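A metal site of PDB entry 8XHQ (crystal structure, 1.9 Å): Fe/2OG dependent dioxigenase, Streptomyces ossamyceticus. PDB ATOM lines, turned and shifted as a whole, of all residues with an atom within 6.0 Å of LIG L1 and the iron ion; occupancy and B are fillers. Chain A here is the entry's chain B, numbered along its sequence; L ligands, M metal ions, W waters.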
ATOM      1  N   ALA A 152      12.399 -14.150  24.904  1.00  0.00           N
ATOM      2  CA  ALA A 152      11.639 -14.115  26.146  1.00  0.00           C
ATOM      3  C   ALA A 152      12.531 -14.569  27.302  1.00  0.00           C
ATOM      4  O   ALA A 152      13.296 -15.533  27.173  1.00  0.00           O
ATOM      5  CB  ALA A 152      10.389 -14.996  26.090  1.00  0.00           C
ATOM      6  N   SER A 154      11.666 -15.617  31.256  1.00  0.00           N
ATOM      7  CA  SER A 154      10.542 -15.850  32.163  1.00  0.00           C
ATOM      8  C   SER A 154      11.006 -16.173  33.572  1.00  0.00           C
ATOM      9  O   SER A 154      11.914 -17.001  33.758  1.00  0.00           O
ATOM     10  CB  SER A 154       9.656 -16.982  31.638  1.00  0.00           C
ATOM     11  OG  SER A 154       9.018 -16.592  30.443  1.00  0.00           O
ATOM     12  N   TYR A 156       9.114 -17.579  37.059  1.00  0.00           N
ATOM     13  CA  TYR A 156       7.892 -18.132  37.645  1.00  0.00           C
ATOM     14  C   TYR A 156       7.827 -17.793  39.121  1.00  0.00           C
ATOM     15  O   TYR A 156       8.553 -18.379  39.933  1.00  0.00           O
ATOM     16  CB  TYR A 156       7.837 -19.636  37.404  1.00  0.00           C
ATOM     17  CG  TYR A 156       7.732 -19.895  35.922  1.00  0.00           C
ATOM     18  CD1 TYR A 156       8.871 -19.949  35.109  1.00  0.00           C
ATOM     19  CD2 TYR A 156       6.477 -20.000  35.318  1.00  0.00           C
ATOM     20  CE1 TYR A 156       8.745 -20.148  33.717  1.00  0.00           C
ATOM     21  CE2 TYR A 156       6.355 -20.207  33.956  1.00  0.00           C
ATOM     22  CZ  TYR A 156       7.475 -20.261  33.159  1.00  0.00           C
ATOM     23  OH  TYR A 156       7.299 -20.447  31.811  1.00  0.00           O
ATOM     24  N   CYS A 165       2.364 -21.014  33.522  1.00  0.00           N
ATOM     25  CA  CYS A 165       2.254 -20.340  32.227  1.00  0.00           C
ATOM     26  C   CYS A 165       0.939 -20.748  31.580  1.00  0.00           C
ATOM     27  O   CYS A 165       0.594 -21.927  31.597  1.00  0.00           O
ATOM     28  CB  CYS A 165       3.422 -20.725  31.284  1.00  0.00           C
ATOM     29  SG  CYS A 165       3.536 -19.812  29.738  1.00  0.00           S
ATOM     30  N   HIS A 168      -0.585 -22.684  25.765  1.00  0.00           N
ATOM     31  CA  HIS A 168      -0.556 -21.977  24.482  1.00  0.00           C
ATOM     32  C   HIS A 168       0.165 -22.811  23.446  1.00  0.00           C
ATOM     33  O   HIS A 168       0.912 -23.743  23.762  1.00  0.00           O
ATOM     34  CB  HIS A 168       0.126 -20.606  24.602  1.00  0.00           C
ATOM     35  CG  HIS A 168       1.554 -20.690  25.049  1.00  0.00           C
ATOM     36  ND1 HIS A 168       1.911 -20.879  26.362  1.00  0.00           N
ATOM     37  CD2 HIS A 168       2.711 -20.612  24.350  1.00  0.00           C
ATOM     38  CE1 HIS A 168       3.221 -20.921  26.465  1.00  0.00           C
ATOM     39  NE2 HIS A 168       3.729 -20.745  25.257  1.00  0.00           N
ATOM     40  N   LYS A 169      -0.065 -22.442  22.193  1.00  0.00           N
ATOM     41  CA  LYS A 169       0.835 -22.748  21.097  1.00  0.00           C
ATOM     42  C   LYS A 169       1.672 -21.521  20.804  1.00  0.00           C
ATOM     43  O   LYS A 169       1.155 -20.413  20.738  1.00  0.00           O
ATOM     44  CB  LYS A 169       0.068 -23.169  19.835  1.00  0.00           C
ATOM     45  CG  LYS A 169      -0.862 -24.389  20.045  1.00  0.00           C
ATOM     46  CD  LYS A 169      -1.599 -24.738  18.713  1.00  0.00           C
ATOM     47  CE  LYS A 169      -2.493 -25.974  18.845  1.00  0.00           C
ATOM     48  NZ  LYS A 169      -3.159 -26.312  17.528  1.00  0.00           N
ATOM     49  N   ASP A 170       2.984 -21.713  20.658  1.00  0.00           N
ATOM     50  CA  ASP A 170       3.829 -20.602  20.231  1.00  0.00           C
ATOM     51  C   ASP A 170       3.290 -20.056  18.906  1.00  0.00           C
ATOM     52  O   ASP A 170       2.606 -20.760  18.168  1.00  0.00           O
ATOM     53  CB  ASP A 170       5.294 -21.063  20.085  1.00  0.00           C
ATOM     54  CG  ASP A 170       5.925 -21.365  21.456  1.00  0.00           C
ATOM     55  OD1 ASP A 170       5.322 -20.957  22.450  1.00  0.00           O
ATOM     56  OD2 ASP A 170       6.976 -21.994  21.529  1.00  0.00           O
ATOM     57  N   THR A 175      10.770 -22.237  17.739  1.00  0.00           N
ATOM     58  CA  THR A 175      11.175 -21.811  19.076  1.00  0.00           C
ATOM     59  C   THR A 175      12.425 -22.582  19.495  1.00  0.00           C
ATOM     60  O   THR A 175      12.502 -23.793  19.287  1.00  0.00           O
ATOM     61  CB  THR A 175      10.062 -22.093  20.094  1.00  0.00           C
ATOM     62  OG1 THR A 175       8.841 -21.472  19.671  1.00  0.00           O
ATOM     63  CG2 THR A 175      10.472 -21.601  21.495  1.00  0.00           C
ATOM     64  N   LEU A 177      14.274 -23.084  23.091  1.00  0.00           N
ATOM     65  CA  LEU A 177      13.975 -22.797  24.492  1.00  0.00           C
ATOM     66  C   LEU A 177      15.032 -23.399  25.409  1.00  0.00           C
ATOM     67  O   LEU A 177      15.412 -24.565  25.243  1.00  0.00           O
ATOM     68  CB  LEU A 177      12.595 -23.339  24.868  1.00  0.00           C
ATOM     69  CG  LEU A 177      12.142 -23.389  26.335  1.00  0.00           C
ATOM     70  CD1 LEU A 177      11.823 -21.996  26.881  1.00  0.00           C
ATOM     71  CD2 LEU A 177      10.930 -24.328  26.522  1.00  0.00           C
ATOM     72  N   ILE A 179      15.511 -24.561  29.269  1.00  0.00           N
ATOM     73  CA  ILE A 179      14.947 -24.868  30.577  1.00  0.00           C
ATOM     74  C   ILE A 179      15.936 -25.720  31.367  1.00  0.00           C
ATOM     75  O   ILE A 179      16.744 -26.465  30.799  1.00  0.00           O
ATOM     76  CB  ILE A 179      13.594 -25.620  30.469  1.00  0.00           C
ATOM     77  CG1 ILE A 179      13.763 -26.854  29.577  1.00  0.00           C
ATOM     78  CG2 ILE A 179      12.503 -24.667  29.947  1.00  0.00           C
ATOM     79  CD1 ILE A 179      12.587 -27.827  29.566  1.00  0.00           C
ATOM     80  N   GLY A 183       8.403 -28.887  34.880  1.00  0.00           N
ATOM     81  CA  GLY A 183       7.275 -27.983  34.959  1.00  0.00           C
ATOM     82  C   GLY A 183       6.611 -27.817  33.607  1.00  0.00           C
ATOM     83  O   GLY A 183       5.391 -27.647  33.526  1.00  0.00           O
ATOM     84  N   LEU A 184       7.396 -27.874  32.549  1.00  0.00           N
ATOM     85  CA  LEU A 184       6.822 -27.798  31.204  1.00  0.00           C
ATOM     86  C   LEU A 184       6.082 -29.091  30.881  1.00  0.00           C
ATOM     87  O   LEU A 184       6.553 -30.186  31.194  1.00  0.00           O
ATOM     88  CB  LEU A 184       7.929 -27.541  30.184  1.00  0.00           C
ATOM     89  CG  LEU A 184       7.501 -27.435  28.728  1.00  0.00           C
ATOM     90  CD1 LEU A 184       6.651 -26.220  28.529  1.00  0.00           C
ATOM     91  CD2 LEU A 184       8.729 -27.373  27.810  1.00  0.00           C
ATOM     92  N   ASN A 205      10.650 -26.371  19.368  1.00  0.00           N
ATOM     93  CA  ASN A 205       9.339 -26.732  18.834  1.00  0.00           C
ATOM     94  C   ASN A 205       8.946 -25.728  17.773  1.00  0.00           C
ATOM     95  O   ASN A 205       9.683 -24.786  17.457  1.00  0.00           O
ATOM     96  CB  ASN A 205       8.272 -26.828  19.945  1.00  0.00           C
ATOM     97  CG  ASN A 205       8.122 -25.549  20.717  1.00  0.00           C
ATOM     98  OD1 ASN A 205       8.765 -25.369  21.737  1.00  0.00           O
ATOM     99  ND2 ASN A 205       7.273 -24.662  20.229  1.00  0.00           N
ATOM    100  N   HIS A 226       1.286 -26.427  24.968  1.00  0.00           N
ATOM    101  CA  HIS A 226       2.115 -26.655  26.135  1.00  0.00           C
ATOM    102  C   HIS A 226       1.807 -25.617  27.190  1.00  0.00           C
ATOM    103  O   HIS A 226       1.309 -24.521  26.908  1.00  0.00           O
ATOM    104  CB  HIS A 226       3.610 -26.647  25.771  1.00  0.00           C
ATOM    105  CG  HIS A 226       4.051 -25.422  25.039  1.00  0.00           C
ATOM    106  ND1 HIS A 226       3.758 -25.202  23.708  1.00  0.00           N
ATOM    107  CD2 HIS A 226       4.784 -24.364  25.446  1.00  0.00           C
ATOM    108  CE1 HIS A 226       4.283 -24.044  23.335  1.00  0.00           C
ATOM    109  NE2 HIS A 226       4.922 -23.523  24.365  1.00  0.00           N
ATOM    110  N   ARG A 227       2.100 -25.988  28.440  1.00  0.00           N
ATOM    111  CA  ARG A 227       1.920 -25.090  29.570  1.00  0.00           C
ATOM    112  C   ARG A 227       3.058 -25.329  30.551  1.00  0.00           C
ATOM    113  O   ARG A 227       3.812 -26.286  30.429  1.00  0.00           O
ATOM    114  CB  ARG A 227       0.565 -25.317  30.258  1.00  0.00           C
ATOM    115  CG  ARG A 227       0.449 -26.692  30.893  1.00  0.00           C
ATOM    116  CD  ARG A 227      -0.842 -26.854  31.714  1.00  0.00           C
ATOM    117  NE  ARG A 227      -0.767 -28.028  32.574  1.00  0.00           N
ATOM    118  CZ  ARG A 227      -1.724 -28.437  33.393  1.00  0.00           C
ATOM    119  NH1 ARG A 227      -1.534 -29.519  34.151  1.00  0.00           N
ATOM    120  NH2 ARG A 227      -2.879 -27.769  33.464  1.00  0.00           N
ATOM    121  N   VAL A 228       3.138 -24.467  31.563  1.00  0.00           N
ATOM    122  CA  VAL A 228       3.946 -24.734  32.747  1.00  0.00           C
ATOM    123  C   VAL A 228       3.008 -24.866  33.938  1.00  0.00           C
ATOM    124  O   VAL A 228       2.259 -23.931  34.262  1.00  0.00           O
ATOM    125  CB  VAL A 228       5.000 -23.635  32.984  1.00  0.00           C
ATOM    126  CG1 VAL A 228       5.817 -23.970  34.220  1.00  0.00           C
ATOM    127  CG2 VAL A 228       5.922 -23.542  31.760  1.00  0.00           C
ATOM    128  N   ARG A 240      11.805 -21.256  39.332  1.00  0.00           N
ATOM    129  CA  ARG A 240      11.898 -21.688  37.949  1.00  0.00           C
ATOM    130  C   ARG A 240      12.038 -20.503  37.022  1.00  0.00           C
ATOM    131  O   ARG A 240      11.427 -19.447  37.221  1.00  0.00           O
ATOM    132  CB  ARG A 240      10.668 -22.506  37.543  1.00  0.00           C
ATOM    133  CG  ARG A 240      10.836 -23.174  36.150  1.00  0.00           C
ATOM    134  CD  ARG A 240       9.704 -24.159  35.870  1.00  0.00           C
ATOM    135  NE  ARG A 240       9.986 -24.978  34.694  1.00  0.00           N
ATOM    136  CZ  ARG A 240       9.846 -24.543  33.448  1.00  0.00           C
ATOM    137  NH1 ARG A 240       9.430 -23.295  33.241  1.00  0.00           N
ATOM    138  NH2 ARG A 240      10.098 -25.341  32.399  1.00  0.00           N
ATOM    139  N   PHE A 241      12.876 -20.659  35.998  1.00  0.00           N
ATOM    140  CA  PHE A 241      12.989 -19.671  34.943  1.00  0.00           C
ATOM    141  C   PHE A 241      13.103 -20.397  33.611  1.00  0.00           C
ATOM    142  O   PHE A 241      13.331 -21.608  33.560  1.00  0.00           O
ATOM    143  CB  PHE A 241      14.197 -18.743  35.159  1.00  0.00           C
ATOM    144  CG  PHE A 241      15.537 -19.440  35.039  1.00  0.00           C
ATOM    145  CD1 PHE A 241      16.136 -19.597  33.806  1.00  0.00           C
ATOM    146  CD2 PHE A 241      16.202 -19.904  36.169  1.00  0.00           C
ATOM    147  CE1 PHE A 241      17.360 -20.223  33.685  1.00  0.00           C
ATOM    148  CE2 PHE A 241      17.418 -20.526  36.077  1.00  0.00           C
ATOM    149  CZ  PHE A 241      18.018 -20.694  34.824  1.00  0.00           C
ATOM    150  N   SER A 242      12.962 -19.647  32.526  1.00  0.00           N
ATOM    151  CA  SER A 242      13.268 -20.147  31.195  1.00  0.00           C
ATOM    152  C   SER A 242      13.597 -18.957  30.312  1.00  0.00           C
ATOM    153  O   SER A 242      13.217 -17.821  30.616  1.00  0.00           O
ATOM    154  CB  SER A 242      12.098 -20.956  30.601  1.00  0.00           C
ATOM    155  OG  SER A 242      11.018 -20.086  30.228  1.00  0.00           O
ATOM    156  N   ALA A 244      14.126 -18.064  25.835  1.00  0.00           N
ATOM    157  CA  ALA A 244      13.865 -18.636  24.529  1.00  0.00           C
ATOM    158  C   ALA A 244      13.960 -17.555  23.476  1.00  0.00           C
ATOM    159  O   ALA A 244      13.766 -16.375  23.765  1.00  0.00           O
ATOM    160  CB  ALA A 244      12.472 -19.290  24.504  1.00  0.00           C
ATOM    161  N   PHE A 246      12.496 -16.909  19.342  1.00  0.00           N
ATOM    162  CA  PHE A 246      11.423 -17.332  18.449  1.00  0.00           C
ATOM    163  C   PHE A 246      11.596 -16.603  17.122  1.00  0.00           C
ATOM    164  O   PHE A 246      11.800 -15.388  17.100  1.00  0.00           O
ATOM    165  CB  PHE A 246      10.019 -17.016  18.995  1.00  0.00           C
ATOM    166  CG  PHE A 246       9.815 -17.283  20.473  1.00  0.00           C
ATOM    167  CD1 PHE A 246      10.307 -16.410  21.432  1.00  0.00           C
ATOM    168  CD2 PHE A 246       9.031 -18.346  20.892  1.00  0.00           C
ATOM    169  CE1 PHE A 246      10.081 -16.643  22.780  1.00  0.00           C
ATOM    170  CE2 PHE A 246       8.797 -18.589  22.235  1.00  0.00           C
ATOM    171  CZ  PHE A 246       9.320 -17.727  23.180  1.00  0.00           C
HETATM  172  C1  LIG L   1       7.548 -19.752  26.038  1.00  0.00           C
HETATM  173  O1  LIG L   1       6.836 -19.558  25.038  1.00  0.00           O
HETATM  174  O2  LIG L   1       8.425 -18.913  26.347  1.00  0.00           O
HETATM  175  C2  LIG L   1       7.348 -20.938  26.882  1.00  0.00           C
HETATM  176  O3  LIG L   1       6.497 -21.763  26.648  1.00  0.00           O
HETATM  177  C3  LIG L   1       8.222 -21.225  28.074  1.00  0.00           C
HETATM  178  C4  LIG L   1       7.813 -22.578  28.694  1.00  0.00           C
HETATM  179  C5  LIG L   1       8.723 -22.833  29.898  1.00  0.00           C
HETATM  180  O4  LIG L   1       9.196 -23.966  30.067  1.00  0.00           O
HETATM  181  O5  LIG L   1       8.971 -21.898  30.700  1.00  0.00           O
HETATM  182  C1  LG2 L   2       4.632 -15.884  21.606  1.00  0.00           C
HETATM  183  C2  LG2 L   2       5.199 -17.301  21.768  1.00  0.00           C
HETATM  184  C3  LG2 L   2       4.716 -17.222  24.283  1.00  0.00           C
HETATM  185  C4  LG2 L   2       3.620 -16.203  23.935  1.00  0.00           C
HETATM  186  C5  LG2 L   2       5.737 -14.813  21.694  1.00  0.00           C
HETATM  187  C6  LG2 L   2       6.846 -15.092  20.687  1.00  0.00           C
HETATM  188  C7  LG2 L   2       5.080 -13.438  21.395  1.00  0.00           C
HETATM  189  C8  LG2 L   2       4.451 -13.370  19.997  1.00  0.00           C
HETATM  190  C9  LG2 L   2       5.871 -16.547  25.062  1.00  0.00           C
HETATM  191  C10 LG2 L   2       5.434 -16.204  26.517  1.00  0.00           C
HETATM  192  C11 LG2 L   2       6.638 -15.451  27.129  1.00  0.00           C
HETATM  193  C12 LG2 L   2       5.154 -17.470  27.342  1.00  0.00           C
HETATM  194  N1  LG2 L   2       3.608 -15.572  22.614  1.00  0.00           N
HETATM  195  N2  LG2 L   2       5.229 -17.912  23.098  1.00  0.00           N
HETATM  196  O1  LG2 L   2       2.763 -15.922  24.728  1.00  0.00           O
HETATM  197  O2  LG2 L   2       5.612 -17.914  20.834  1.00  0.00           O
HETATM  198  O3  LG2 L   2       3.122 -13.865  19.996  1.00  0.00           O
HETATM  199 FE    FE M   1       5.738 -21.471  24.568  1.00  0.00          FE
HETATM  200  O   HOH W   1       7.760 -22.416  23.979  1.00  0.00           O
HETATM  201  O   HOH W   2      10.200 -18.097  28.331  1.00  0.00           O
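Three residues have an atom within 4 Å of the iron ion: His 168, Asp 170 and His 226. The nearest printed residue that does not touch the iron ion is Phe 246 (4.8 Å).
OH of Tyr 156 sits at hydrogen-bond distance from O5 of LIG L1, at 2.5 Å. The side-chain hydroxyl of Ser 242 sits at hydrogen-bond distance from an oxygen (O5) of LIG L1, at 2.8 Å. NH2 of Arg 240 is in salt-bridge range of O4 of LIG L1 (2.9 Å). OD1 of Asp 170 lies close to N2 of LG2 L2 (3.1 Å).
The side-chain carboxylate (OD2) of Asp 170 is in hydrogen-bond range of the side-chain hydroxyl (OG1) of Thr 175 (2.7 Å). The side-chain amide nitrogen of Asn 205 lies within hydrogen-bond range of the side-chain carboxylate of Asp 170. The backbone carbonyl oxygen (O) of Arg 240 is in hydrogen-bond range of the backbone NH (N) of Tyr 156 (3.0 Å). O of Ser 242 lies within hydrogen-bond range of N of Ser 154, at 2.8 Å. The backbone carbonyl oxygen (O) of Val 228 lies within hydrogen-bond range of the backbone NH (N) of Cys 165 (3.0 Å).
Water W2 lies within hydrogen-bond range of an oxygen (O2) of LIG L1, the side-chain hydroxyl of Ser 154 and the side-chain hydroxyl of Ser 242.
The iron ion is bound by NE2 of His 226, OD1 of Asp 170, O3 of LIG L1, NE2 of His 168, O1 of LIG L1 and water W1. The iron ion has six donor atoms within binding distance.
O1 of LIG L1 lies close to N2 of LG2 L2, at 3.0 Å.
Residues that only touch LIG L1: Leu 177, Ile 179, Leu 184, Val 228 and Phe 246. Hydrophobic or aromatic side chains that line LIG L1: Tyr 156, His 168, Leu 177, Ile 179, Leu 184, His 226, Val 228 and Phe 246. Of the 21 residues printed, 11 come within 4 Å of LIG L1. The nearest printed residue that does not touch LIG L1 is Ala 152 (4.4 Å).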
